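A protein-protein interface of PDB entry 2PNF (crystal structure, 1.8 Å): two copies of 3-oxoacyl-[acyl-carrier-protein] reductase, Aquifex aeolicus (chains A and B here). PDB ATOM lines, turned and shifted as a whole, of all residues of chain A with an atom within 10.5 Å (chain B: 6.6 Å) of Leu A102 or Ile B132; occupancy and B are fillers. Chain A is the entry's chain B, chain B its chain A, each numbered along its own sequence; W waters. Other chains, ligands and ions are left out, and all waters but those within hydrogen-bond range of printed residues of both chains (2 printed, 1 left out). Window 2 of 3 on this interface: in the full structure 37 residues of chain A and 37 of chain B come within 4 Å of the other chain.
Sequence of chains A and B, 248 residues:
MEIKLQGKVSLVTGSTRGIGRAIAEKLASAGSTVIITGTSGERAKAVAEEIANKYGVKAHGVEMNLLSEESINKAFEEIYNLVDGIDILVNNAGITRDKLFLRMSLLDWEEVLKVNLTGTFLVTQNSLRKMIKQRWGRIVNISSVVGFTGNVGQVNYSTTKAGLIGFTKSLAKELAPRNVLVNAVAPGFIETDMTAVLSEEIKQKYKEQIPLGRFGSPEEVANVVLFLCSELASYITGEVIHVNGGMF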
ATOM      1  N   ARG A  97      21.193   8.399 -15.703  1.00  0.00           N
ATOM      2  CA  ARG A  97      19.738   8.307 -15.641  1.00  0.00           C
ATOM      3  C   ARG A  97      19.431   9.689 -15.108  1.00  0.00           C
ATOM      4  O   ARG A  97      19.120   9.865 -13.927  1.00  0.00           O
ATOM      5  CB  ARG A  97      19.273   7.227 -14.669  1.00  0.00           C
ATOM      6  CG  ARG A  97      19.527   5.781 -15.133  1.00  0.00           C
ATOM      7  CD  ARG A  97      18.796   5.426 -16.451  1.00  0.00           C
ATOM      8  NE  ARG A  97      19.104   4.061 -16.910  1.00  0.00           N
ATOM      9  CZ  ARG A  97      20.003   3.745 -17.851  1.00  0.00           C
ATOM     10  NH1 ARG A  97      20.713   4.693 -18.471  1.00  0.00           N
ATOM     11  NH2 ARG A  97      20.206   2.465 -18.173  1.00  0.00           N
ATOM     12  N   ASP A  98      19.544  10.679 -15.996  1.00  0.00           N
ATOM     13  CA  ASP A  98      19.377  12.074 -15.598  1.00  0.00           C
ATOM     14  C   ASP A  98      17.965  12.425 -15.232  1.00  0.00           C
ATOM     15  O   ASP A  98      17.043  12.165 -15.993  1.00  0.00           O
ATOM     16  CB  ASP A  98      19.872  13.050 -16.683  1.00  0.00           C
ATOM     17  CG  ASP A  98      21.327  12.799 -17.095  1.00  0.00           C
ATOM     18  OD1 ASP A  98      22.121  12.294 -16.271  1.00  0.00           O
ATOM     19  OD2 ASP A  98      21.685  13.117 -18.254  1.00  0.00           O
ATOM     20  N   LYS A  99      17.810  13.032 -14.064  1.00  0.00           N
ATOM     21  CA  LYS A  99      16.505  13.451 -13.557  1.00  0.00           C
ATOM     22  C   LYS A  99      16.761  14.514 -12.512  1.00  0.00           C
ATOM     23  O   LYS A  99      17.777  14.451 -11.819  1.00  0.00           O
ATOM     24  CB  LYS A  99      15.784  12.312 -12.831  1.00  0.00           C
ATOM     25  CG  LYS A  99      15.238  11.205 -13.700  1.00  0.00           C
ATOM     26  CD  LYS A  99      14.026  11.662 -14.483  1.00  0.00           C
ATOM     27  CE  LYS A  99      13.407  10.488 -15.229  1.00  0.00           C
ATOM     28  NZ  LYS A  99      12.238  10.891 -16.069  1.00  0.00           N
ATOM     29  N   LEU A 100      15.864  15.496 -12.401  1.00  0.00           N
ATOM     30  CA  LEU A 100      16.019  16.477 -11.324  1.00  0.00           C
ATOM     31  C   LEU A 100      15.794  15.633 -10.066  1.00  0.00           C
ATOM     32  O   LEU A 100      15.018  14.683 -10.081  1.00  0.00           O
ATOM     33  CB  LEU A 100      14.954  17.575 -11.395  1.00  0.00           C
ATOM     34  CG  LEU A 100      15.073  18.636 -12.491  1.00  0.00           C
ATOM     35  CD1 LEU A 100      13.885  19.608 -12.389  1.00  0.00           C
ATOM     36  CD2 LEU A 100      16.391  19.393 -12.334  1.00  0.00           C
ATOM     37  N   PHE A 101      16.466  15.982  -8.966  1.00  0.00           N
ATOM     38  CA  PHE A 101      16.376  15.208  -7.740  1.00  0.00           C
ATOM     39  C   PHE A 101      14.943  14.951  -7.277  1.00  0.00           C
ATOM     40  O   PHE A 101      14.581  13.838  -6.891  1.00  0.00           O
ATOM     41  CB  PHE A 101      17.160  15.918  -6.619  1.00  0.00           C
ATOM     42  CG  PHE A 101      17.283  15.098  -5.378  1.00  0.00           C
ATOM     43  CD1 PHE A 101      18.210  14.068  -5.302  1.00  0.00           C
ATOM     44  CD2 PHE A 101      16.479  15.355  -4.275  1.00  0.00           C
ATOM     45  CE1 PHE A 101      18.331  13.324  -4.157  1.00  0.00           C
ATOM     46  CE2 PHE A 101      16.590  14.612  -3.120  1.00  0.00           C
ATOM     47  CZ  PHE A 101      17.515  13.596  -3.054  1.00  0.00           C
ATOM     48  N   LEU A 102      14.130  15.990  -7.329  1.00  0.00           N
ATOM     49  CA  LEU A 102      12.742  15.878  -6.895  1.00  0.00           C
ATOM     50  C   LEU A 102      11.943  14.955  -7.815  1.00  0.00           C
ATOM     51  O   LEU A 102      10.837  14.543  -7.467  1.00  0.00           O
ATOM     52  CB  LEU A 102      12.102  17.269  -6.862  1.00  0.00           C
ATOM     53  CG  LEU A 102      12.538  18.088  -5.639  1.00  0.00           C
ATOM     54  CD1 LEU A 102      12.348  19.589  -5.909  1.00  0.00           C
ATOM     55  CD2 LEU A 102      11.754  17.613  -4.410  1.00  0.00           C
ATOM     56  N   ARG A 103      12.497  14.645  -8.985  1.00  0.00           N
ATOM     57  CA  ARG A 103      11.821  13.757  -9.932  1.00  0.00           C
ATOM     58  C   ARG A 103      12.544  12.427 -10.057  1.00  0.00           C
ATOM     59  O   ARG A 103      12.204  11.627 -10.911  1.00  0.00           O
ATOM     60  CB  ARG A 103      11.785  14.375 -11.334  1.00  0.00           C
ATOM     61  CG  ARG A 103      11.287  15.827 -11.399  1.00  0.00           C
ATOM     62  CD  ARG A 103       9.928  15.961 -10.788  1.00  0.00           C
ATOM     63  NE  ARG A 103       9.010  15.007 -11.388  1.00  0.00           N
ATOM     64  CZ  ARG A 103       8.172  14.259 -10.689  1.00  0.00           C
ATOM     65  NH1 ARG A 103       8.145  14.361  -9.365  1.00  0.00           N
ATOM     66  NH2 ARG A 103       7.357  13.422 -11.323  1.00  0.00           N
ATOM     67  N   MET A 104      13.534  12.169  -9.214  1.00  0.00           N
ATOM     68  CA  MET A 104      14.307  10.931  -9.350  1.00  0.00           C
ATOM     69  C   MET A 104      13.722   9.718  -8.654  1.00  0.00           C
ATOM     70  O   MET A 104      13.430   9.754  -7.463  1.00  0.00           O
ATOM     71  CB  MET A 104      15.747  11.205  -8.859  1.00  0.00           C
ATOM     72  CG  MET A 104      16.713  10.077  -9.155  1.00  0.00           C
ATOM     73  SD  MET A 104      18.426  10.614  -8.673  1.00  0.00           S
ATOM     74  CE  MET A 104      18.765  11.762 -10.003  1.00  0.00           C
ATOM     75  N   SER A 105      13.555   8.613  -9.389  1.00  0.00           N
ATOM     76  CA  SER A 105      12.987   7.416  -8.790  1.00  0.00           C
ATOM     77  C   SER A 105      14.090   6.611  -8.121  1.00  0.00           C
ATOM     78  O   SER A 105      15.274   6.816  -8.410  1.00  0.00           O
ATOM     79  CB  SER A 105      12.318   6.546  -9.856  1.00  0.00           C
ATOM     80  OG  SER A 105      13.285   5.855 -10.625  1.00  0.00           O
ATOM     81  N   LEU A 106      13.706   5.704  -7.225  1.00  0.00           N
ATOM     82  CA  LEU A 106      14.686   4.855  -6.565  1.00  0.00           C
ATOM     83  C   LEU A 106      15.459   4.045  -7.606  1.00  0.00           C
ATOM     84  O   LEU A 106      16.661   3.831  -7.465  1.00  0.00           O
ATOM     85  CB  LEU A 106      14.000   3.925  -5.559  1.00  0.00           C
ATOM     86  CG  LEU A 106      14.959   3.110  -4.665  1.00  0.00           C
ATOM     87  CD1 LEU A 106      15.865   4.062  -3.858  1.00  0.00           C
ATOM     88  CD2 LEU A 106      14.149   2.217  -3.713  1.00  0.00           C
ATOM     89  N   ASP A 108      16.100   5.018 -10.708  1.00  0.00           N
ATOM     90  CA  ASP A 108      16.968   5.954 -11.425  1.00  0.00           C
ATOM     91  C   ASP A 108      18.252   6.064 -10.593  1.00  0.00           C
ATOM     92  O   ASP A 108      19.346   6.168 -11.122  1.00  0.00           O
ATOM     93  CB  ASP A 108      16.398   7.373 -11.513  1.00  0.00           C
ATOM     94  CG  ASP A 108      15.246   7.516 -12.510  1.00  0.00           C
ATOM     95  OD1 ASP A 108      15.252   6.803 -13.548  1.00  0.00           O
ATOM     96  OD2 ASP A 108      14.370   8.382 -12.244  1.00  0.00           O
ATOM     97  N   TRP A 109      18.085   6.087  -9.281  1.00  0.00           N
ATOM     98  CA  TRP A 109      19.244   6.174  -8.397  1.00  0.00           C
ATOM     99  C   TRP A 109      20.017   4.869  -8.265  1.00  0.00           C
ATOM    100  O   TRP A 109      21.221   4.829  -8.512  1.00  0.00           O
ATOM    101  CB  TRP A 109      18.799   6.652  -7.009  1.00  0.00           C
ATOM    102  CG  TRP A 109      19.907   6.618  -5.969  1.00  0.00           C
ATOM    103  CD1 TRP A 109      20.237   5.579  -5.152  1.00  0.00           C
ATOM    104  CD2 TRP A 109      20.791   7.695  -5.630  1.00  0.00           C
ATOM    105  NE1 TRP A 109      21.281   5.949  -4.319  1.00  0.00           N
ATOM    106  CE2 TRP A 109      21.632   7.241  -4.591  1.00  0.00           C
ATOM    107  CE3 TRP A 109      20.950   9.002  -6.105  1.00  0.00           C
ATOM    108  CZ2 TRP A 109      22.614   8.058  -4.016  1.00  0.00           C
ATOM    109  CZ3 TRP A 109      21.932   9.818  -5.535  1.00  0.00           C
ATOM    110  CH2 TRP A 109      22.745   9.336  -4.500  1.00  0.00           C
ATOM    111  N   VAL A 152      23.392  19.901 -12.103  1.00  0.00           N
ATOM    112  CA  VAL A 152      21.942  19.822 -12.038  1.00  0.00           C
ATOM    113  C   VAL A 152      21.423  18.653 -12.915  1.00  0.00           C
ATOM    114  O   VAL A 152      21.898  18.445 -14.052  1.00  0.00           O
ATOM    115  CB  VAL A 152      21.294  21.161 -12.506  1.00  0.00           C
ATOM    116  CG1 VAL A 152      19.757  21.019 -12.587  1.00  0.00           C
ATOM    117  CG2 VAL A 152      21.650  22.250 -11.521  1.00  0.00           C
ATOM    118  N   GLY A 153      20.469  17.893 -12.384  1.00  0.00           N
ATOM    119  CA  GLY A 153      19.902  16.781 -13.123  1.00  0.00           C
ATOM    120  C   GLY A 153      20.738  15.517 -13.010  1.00  0.00           C
ATOM    121  O   GLY A 153      20.340  14.451 -13.488  1.00  0.00           O
ATOM    122  N   GLN A 154      21.895  15.640 -12.355  1.00  0.00           N
ATOM    123  CA  GLN A 154      22.797  14.510 -12.211  1.00  0.00           C
ATOM    124  C   GLN A 154      23.227  14.177 -10.790  1.00  0.00           C
ATOM    125  O   GLN A 154      24.369  13.784 -10.569  1.00  0.00           O
ATOM    126  CB  GLN A 154      24.041  14.750 -13.087  1.00  0.00           C
ATOM    127  CG  GLN A 154      23.697  14.743 -14.577  1.00  0.00           C
ATOM    128  CD  GLN A 154      24.914  14.558 -15.445  1.00  0.00           C
ATOM    129  OE1 GLN A 154      25.896  15.315 -15.336  1.00  0.00           O
ATOM    130  NE2 GLN A 154      24.863  13.562 -16.325  1.00  0.00           N
ATOM    131  N   VAL A 155      22.326  14.292  -9.825  1.00  0.00           N
ATOM    132  CA  VAL A 155      22.737  13.977  -8.455  1.00  0.00           C
ATOM    133  C   VAL A 155      23.212  12.514  -8.324  1.00  0.00           C
ATOM    134  O   VAL A 155      24.209  12.224  -7.619  1.00  0.00           O
ATOM    135  CB  VAL A 155      21.618  14.286  -7.446  1.00  0.00           C
ATOM    136  CG1 VAL A 155      22.082  13.869  -6.047  1.00  0.00           C
ATOM    137  CG2 VAL A 155      21.333  15.748  -7.436  1.00  0.00           C
ATOM    138  N   ASN A 156      22.545  11.593  -9.028  1.00  0.00           N
ATOM    139  CA  ASN A 156      22.956  10.178  -9.005  1.00  0.00           C
ATOM    140  C   ASN A 156      24.317   9.958  -9.675  1.00  0.00           C
ATOM    141  O   ASN A 156      25.221   9.337  -9.096  1.00  0.00           O
ATOM    142  CB  ASN A 156      21.880   9.246  -9.661  1.00  0.00           C
ATOM    143  CG  ASN A 156      21.355   9.761 -11.026  1.00  0.00           C
ATOM    144  OD1 ASN A 156      21.731  10.841 -11.507  1.00  0.00           O
ATOM    145  ND2 ASN A 156      20.458   8.976 -11.648  1.00  0.00           N
ATOM    146  N   GLN B 125      15.145  12.829   0.057  1.00  0.00           N
ATOM    147  CA  GLN B 125      13.974  13.066  -0.809  1.00  0.00           C
ATOM    148  C   GLN B 125      12.668  13.220   0.007  1.00  0.00           C
ATOM    149  O   GLN B 125      11.796  14.057  -0.300  1.00  0.00           O
ATOM    150  CB  GLN B 125      13.825  11.952  -1.839  1.00  0.00           C
ATOM    151  CG  GLN B 125      13.139  12.493  -3.103  1.00  0.00           C
ATOM    152  CD  GLN B 125      12.998  11.432  -4.169  1.00  0.00           C
ATOM    153  OE1 GLN B 125      12.442  10.360  -3.913  1.00  0.00           O
ATOM    154  NE2 GLN B 125      13.500  11.722  -5.372  1.00  0.00           N
ATOM    155  N   SER B 127      12.436  14.386   3.053  1.00  0.00           N
ATOM    156  CA  SER B 127      12.480  15.520   3.976  1.00  0.00           C
ATOM    157  C   SER B 127      12.331  16.886   3.312  1.00  0.00           C
ATOM    158  O   SER B 127      12.178  17.880   3.995  1.00  0.00           O
ATOM    159  CB  SER B 127      13.823  15.491   4.731  1.00  0.00           C
ATOM    160  OG  SER B 127      14.007  14.268   5.436  1.00  0.00           O
ATOM    161  N   LEU B 128      12.367  16.948   1.983  1.00  0.00           N
ATOM    162  CA  LEU B 128      12.330  18.245   1.321  1.00  0.00           C
ATOM    163  C   LEU B 128      11.070  19.106   1.257  1.00  0.00           C
ATOM    164  O   LEU B 128      11.159  20.326   1.146  1.00  0.00           O
ATOM    165  CB  LEU B 128      12.847  18.065  -0.103  1.00  0.00           C
ATOM    166  CG  LEU B 128      14.352  17.784  -0.169  1.00  0.00           C
ATOM    167  CD1 LEU B 128      14.734  17.460  -1.608  1.00  0.00           C
ATOM    168  CD2 LEU B 128      15.118  19.011   0.318  1.00  0.00           C
ATOM    169  N   ARG B 129       9.909  18.471   1.339  1.00  0.00           N
ATOM    170  CA  ARG B 129       8.638  19.174   1.181  1.00  0.00           C
ATOM    171  C   ARG B 129       8.493  20.550   1.837  1.00  0.00           C
ATOM    172  O   ARG B 129       8.305  21.548   1.149  1.00  0.00           O
ATOM    173  CB  ARG B 129       7.516  18.254   1.649  1.00  0.00           C
ATOM    174  CG  ARG B 129       6.135  18.795   1.438  1.00  0.00           C
ATOM    175  CD  ARG B 129       5.171  17.717   1.863  1.00  0.00           C
ATOM    176  NE  ARG B 129       3.787  18.145   1.805  1.00  0.00           N
ATOM    177  CZ  ARG B 129       2.769  17.360   2.126  1.00  0.00           C
ATOM    178  NH1 ARG B 129       3.005  16.112   2.522  1.00  0.00           N
ATOM    179  NH2 ARG B 129       1.528  17.822   2.058  1.00  0.00           N
ATOM    180  N   LYS B 130       8.570  20.608   3.158  1.00  0.00           N
ATOM    181  CA  LYS B 130       8.409  21.881   3.864  1.00  0.00           C
ATOM    182  C   LYS B 130       9.489  22.906   3.520  1.00  0.00           C
ATOM    183  O   LYS B 130       9.222  24.103   3.418  1.00  0.00           O
ATOM    184  CB  LYS B 130       8.361  21.622   5.375  1.00  0.00           C
ATOM    185  CG  LYS B 130       8.004  22.858   6.232  1.00  0.00           C
ATOM    186  CD  LYS B 130       7.820  22.453   7.690  1.00  0.00           C
ATOM    187  CE  LYS B 130       7.235  23.595   8.544  1.00  0.00           C
ATOM    188  NZ  LYS B 130       8.188  24.738   8.776  1.00  0.00           N
ATOM    189  N   MET B 131      10.713  22.430   3.299  1.00  0.00           N
ATOM    190  CA  MET B 131      11.829  23.288   2.970  1.00  0.00           C
ATOM    191  C   MET B 131      11.628  24.039   1.666  1.00  0.00           C
ATOM    192  O   MET B 131      11.861  25.233   1.593  1.00  0.00           O
ATOM    193  CB  MET B 131      13.140  22.469   2.866  1.00  0.00           C
ATOM    194  CG  MET B 131      13.525  21.712   4.137  1.00  0.00           C
ATOM    195  SD  MET B 131      15.087  20.808   3.819  1.00  0.00           S
ATOM    196  CE  MET B 131      15.150  19.651   5.223  1.00  0.00           C
ATOM    197  N   ILE B 132      11.258  23.307   0.621  1.00  0.00           N
ATOM    198  CA  ILE B 132      11.054  23.889  -0.685  1.00  0.00           C
ATOM    199  C   ILE B 132       9.853  24.839  -0.686  1.00  0.00           C
ATOM    200  O   ILE B 132       9.893  25.910  -1.287  1.00  0.00           O
ATOM    201  CB  ILE B 132      10.879  22.755  -1.710  1.00  0.00           C
ATOM    202  CG1 ILE B 132      12.239  22.057  -1.877  1.00  0.00           C
ATOM    203  CG2 ILE B 132      10.427  23.286  -3.056  1.00  0.00           C
ATOM    204  CD1 ILE B 132      12.154  20.766  -2.629  1.00  0.00           C
ATOM    205  N   LYS B 133       8.820  24.459   0.041  1.00  0.00           N
ATOM    206  CA  LYS B 133       7.615  25.264   0.127  1.00  0.00           C
ATOM    207  C   LYS B 133       7.897  26.610   0.774  1.00  0.00           C
ATOM    208  O   LYS B 133       7.494  27.647   0.246  1.00  0.00           O
ATOM    209  CB  LYS B 133       6.549  24.484   0.915  1.00  0.00           C
ATOM    210  CG  LYS B 133       5.159  25.136   0.958  1.00  0.00           C
ATOM    211  CD  LYS B 133       4.159  24.253   1.702  1.00  0.00           C
ATOM    212  CE  LYS B 133       2.881  25.028   2.079  1.00  0.00           C
ATOM    213  NZ  LYS B 133       1.848  24.137   2.691  1.00  0.00           N
ATOM    214  N   GLN B 134       8.638  26.618   1.887  1.00  0.00           N
ATOM    215  CA  GLN B 134       8.906  27.876   2.596  1.00  0.00           C
ATOM    216  C   GLN B 134      10.175  28.601   2.151  1.00  0.00           C
ATOM    217  O   GLN B 134      10.455  29.700   2.617  1.00  0.00           O
ATOM    218  CB  GLN B 134       8.962  27.609   4.111  1.00  0.00           C
ATOM    219  CG  GLN B 134      10.259  26.959   4.566  1.00  0.00           C
ATOM    220  CD  GLN B 134      10.132  26.243   5.888  1.00  0.00           C
ATOM    221  OE1 GLN B 134       9.074  26.269   6.522  1.00  0.00           O
ATOM    222  NE2 GLN B 134      11.215  25.585   6.325  1.00  0.00           N
ATOM    223  N   ARG B 135      10.921  27.986   1.230  1.00  0.00           N
ATOM    224  CA  ARG B 135      12.170  28.538   0.748  1.00  0.00           C
ATOM    225  C   ARG B 135      13.175  28.758   1.857  1.00  0.00           C
ATOM    226  O   ARG B 135      13.811  29.809   1.948  1.00  0.00           O
ATOM    227  CB  ARG B 135      11.943  29.820  -0.043  1.00  0.00           C
ATOM    228  CG  ARG B 135      11.198  29.485  -1.332  1.00  0.00           C
ATOM    229  CD  ARG B 135      10.972  30.658  -2.243  1.00  0.00           C
ATOM    230  NE  ARG B 135      10.618  30.131  -3.564  1.00  0.00           N
ATOM    231  CZ  ARG B 135      10.098  30.835  -4.565  1.00  0.00           C
ATOM    232  NH1 ARG B 135       9.846  32.136  -4.428  1.00  0.00           N
ATOM    233  NH2 ARG B 135       9.836  30.230  -5.715  1.00  0.00           N
ATOM    234  N   TRP B 136      13.291  27.758   2.712  1.00  0.00           N
ATOM    235  CA  TRP B 136      14.293  27.784   3.773  1.00  0.00           C
ATOM    236  C   TRP B 136      14.446  26.342   4.153  1.00  0.00           C
ATOM    237  O   TRP B 136      13.451  25.639   4.374  1.00  0.00           O
ATOM    238  CB  TRP B 136      13.850  28.585   5.010  1.00  0.00           C
ATOM    239  CG  TRP B 136      15.007  28.850   5.936  1.00  0.00           C
ATOM    240  CD1 TRP B 136      15.768  29.979   5.991  1.00  0.00           C
ATOM    241  CD2 TRP B 136      15.553  27.945   6.925  1.00  0.00           C
ATOM    242  NE1 TRP B 136      16.757  29.844   6.970  1.00  0.00           N
ATOM    243  CE2 TRP B 136      16.643  28.608   7.547  1.00  0.00           C
ATOM    244  CE3 TRP B 136      15.220  26.648   7.345  1.00  0.00           C
ATOM    245  CZ2 TRP B 136      17.404  28.012   8.571  1.00  0.00           C
ATOM    246  CZ3 TRP B 136      15.980  26.051   8.371  1.00  0.00           C
ATOM    247  CH2 TRP B 136      17.058  26.741   8.967  1.00  0.00           C
ATOM    248  N   GLY B 137      15.694  25.875   4.168  1.00  0.00           N
ATOM    249  CA  GLY B 137      15.928  24.491   4.553  1.00  0.00           C
ATOM    250  C   GLY B 137      17.421  24.301   4.675  1.00  0.00           C
ATOM    251  O   GLY B 137      18.180  25.026   4.039  1.00  0.00           O
ATOM    252  N   LEU B 171      23.231  18.434  -5.363  1.00  0.00           N
ATOM    253  CA  LEU B 171      21.948  18.770  -4.761  1.00  0.00           C
ATOM    254  C   LEU B 171      21.927  20.241  -4.362  1.00  0.00           C
ATOM    255  O   LEU B 171      20.895  20.920  -4.471  1.00  0.00           O
ATOM    256  CB  LEU B 171      21.675  17.868  -3.549  1.00  0.00           C
ATOM    257  CG  LEU B 171      20.254  18.077  -2.961  1.00  0.00           C
ATOM    258  CD1 LEU B 171      19.187  17.774  -4.039  1.00  0.00           C
ATOM    259  CD2 LEU B 171      20.067  17.196  -1.753  1.00  0.00           C
ATOM    260  N   GLU B 174      20.927  22.242  -7.394  1.00  0.00           N
ATOM    261  CA  GLU B 174      19.506  22.110  -7.727  1.00  0.00           C
ATOM    262  C   GLU B 174      18.562  22.829  -6.795  1.00  0.00           C
ATOM    263  O   GLU B 174      17.531  23.391  -7.234  1.00  0.00           O
ATOM    264  CB  GLU B 174      19.107  20.664  -7.771  1.00  0.00           C
ATOM    265  CG  GLU B 174      19.592  19.997  -9.020  1.00  0.00           C
ATOM    266  CD  GLU B 174      18.965  18.634  -9.217  1.00  0.00           C
ATOM    267  OE1 GLU B 174      17.906  18.361  -8.576  1.00  0.00           O
ATOM    268  OE2 GLU B 174      19.551  17.861 -10.009  1.00  0.00           O
ATOM    269  N   LEU B 175      18.909  22.810  -5.510  1.00  0.00           N
ATOM    270  CA  LEU B 175      18.050  23.441  -4.520  1.00  0.00           C
ATOM    271  C   LEU B 175      18.346  24.882  -4.178  1.00  0.00           C
ATOM    272  O   LEU B 175      17.559  25.511  -3.491  1.00  0.00           O
ATOM    273  CB  LEU B 175      18.047  22.615  -3.225  1.00  0.00           C
ATOM    274  CG  LEU B 175      17.673  21.139  -3.374  1.00  0.00           C
ATOM    275  CD1 LEU B 175      17.673  20.479  -2.010  1.00  0.00           C
ATOM    276  CD2 LEU B 175      16.292  21.032  -4.033  1.00  0.00           C
ATOM    277  N   ARG B 178      15.787  27.694  -4.428  1.00  0.00           N
ATOM    278  CA  ARG B 178      14.756  27.611  -3.384  1.00  0.00           C
ATOM    279  C   ARG B 178      15.286  27.951  -2.001  1.00  0.00           C
ATOM    280  O   ARG B 178      14.585  27.797  -1.016  1.00  0.00           O
ATOM    281  CB  ARG B 178      14.162  26.208  -3.345  1.00  0.00           C
ATOM    282  CG  ARG B 178      13.267  25.885  -4.533  1.00  0.00           C
ATOM    283  CD  ARG B 178      12.029  26.752  -4.444  1.00  0.00           C
ATOM    284  NE  ARG B 178      11.035  26.427  -5.456  1.00  0.00           N
ATOM    285  CZ  ARG B 178       9.729  26.656  -5.316  1.00  0.00           C
ATOM    286  NH1 ARG B 178       9.260  27.216  -4.194  1.00  0.00           N
ATOM    287  NH2 ARG B 178       8.891  26.315  -6.297  1.00  0.00           N
ATOM    288  N   VAL B 180      17.466  26.390  -0.171  1.00  0.00           N
ATOM    289  CA  VAL B 180      17.595  25.215   0.694  1.00  0.00           C
ATOM    290  C   VAL B 180      19.101  24.924   0.521  1.00  0.00           C
ATOM    291  O   VAL B 180      19.550  24.553  -0.582  1.00  0.00           O
ATOM    292  CB  VAL B 180      16.779  24.040   0.180  1.00  0.00           C
ATOM    293  CG1 VAL B 180      17.035  22.762   1.049  1.00  0.00           C
ATOM    294  CG2 VAL B 180      15.283  24.398   0.262  1.00  0.00           C
HETATM  295  O   HOH W   1      15.258  18.716  -7.735  1.00  0.00           O
HETATM  296  O   HOH W   2      12.298   8.314  -5.259  1.00  0.00           O
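The backbone NH (N) of Gly A153 lies within hydrogen-bond range of the side-chain carboxylate (OE2) of Glu B174, at 2.5 Å. The side-chain amide nitrogen (NE2) of Gln B125 lies within hydrogen-bond range of the backbone carbonyl oxygen (O) of Phe A101. O of Met A104 sits at hydrogen-bond distance from NE2 of Gln B125, 2.9 Å away. N of Phe A101 lies within hydrogen-bond range of OE1 of Glu B174 (2.8 Å).
The backbone carbonyl oxygen (O) of Ile B132 is in hydrogen-bond range of the guanidinium group (NH1) of Arg B178. The side-chain carboxylate of Asp A98 lies within hydrogen-bond range of the side-chain amide nitrogen of Gln A154. The backbone carbonyl oxygen (O) of Gly A153 sits at hydrogen-bond distance from the backbone NH (N) of Lys A99 (3.0 Å).
Among the printed residues, merely in contact across the chains: Leu A102 with Ile B132, Val A152 with Glu B174, Phe A101 with Leu B171, Phe A101 with Leu B128, Leu A100 with Glu B174, Val A155 with Glu B174, Val A155 with Leu B171 and Gln A154 with Glu B174.
Arg A97 touches none of the printed residues of chain B. Leu A102 touches one residue of chain B. Of the printed residues of chain B, Gln A154 touches Glu B174. Printed residues of chain B within 4 Å of Val A155: Leu B171 (3.9 Å) and Glu B174 (3.8 Å). Ile B132 touches just one residue of chain A: Leu A102 (3.5 Å). Printed residues of chain A within 4 Å of Glu B174: Leu A100, Phe A101, Val A152, Gly A153, Gln A154 and Val A155. Leu B175 touches none of the printed residues of chain A. The nearest printed residue of chain A that does not touch Glu B174 is Lys A99 (4.2 Å).
Of the 17 printed residues of chain A, 8 touch a printed residue of chain B. Hydrophobic or aromatic side chains of chain A that line the printed part of chain B: Phe A101, Leu A102, Val A152 and Val A155. Of the 17 printed residues of chain B, 5 touch a printed residue of chain A. Printed residues of chain B that touch a printed residue of chain A: Gln B125, Leu B128, Ile B132, Leu B171 and Glu B174. Hydrophobic or aromatic side chains of chain B within 4 Å of the printed part of chain A: Leu B128, Ile B132 and Leu B171. Among the printed residues, 12 pairs touch across the chains. Among the printed residues, no Asp or Glu carboxylate lies within 4 Å of a Lys or Arg side-chain nitrogen of the other chain.
No position is printed for both chains. Of the 12 pairs that touch across the chains among the printed residues, none has its exchanged pair printed and touching as well.
Water W2 lies within hydrogen-bond range of OE1 of Gln B125 (2.5 Å) and O of Met A104 (2.9 Å). Water W1 lies within hydrogen-bond range of OE1 of Glu B174 (2.8 Å), N of Leu A102 (3.0 Å) and N of Phe A101 (3.2 Å).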
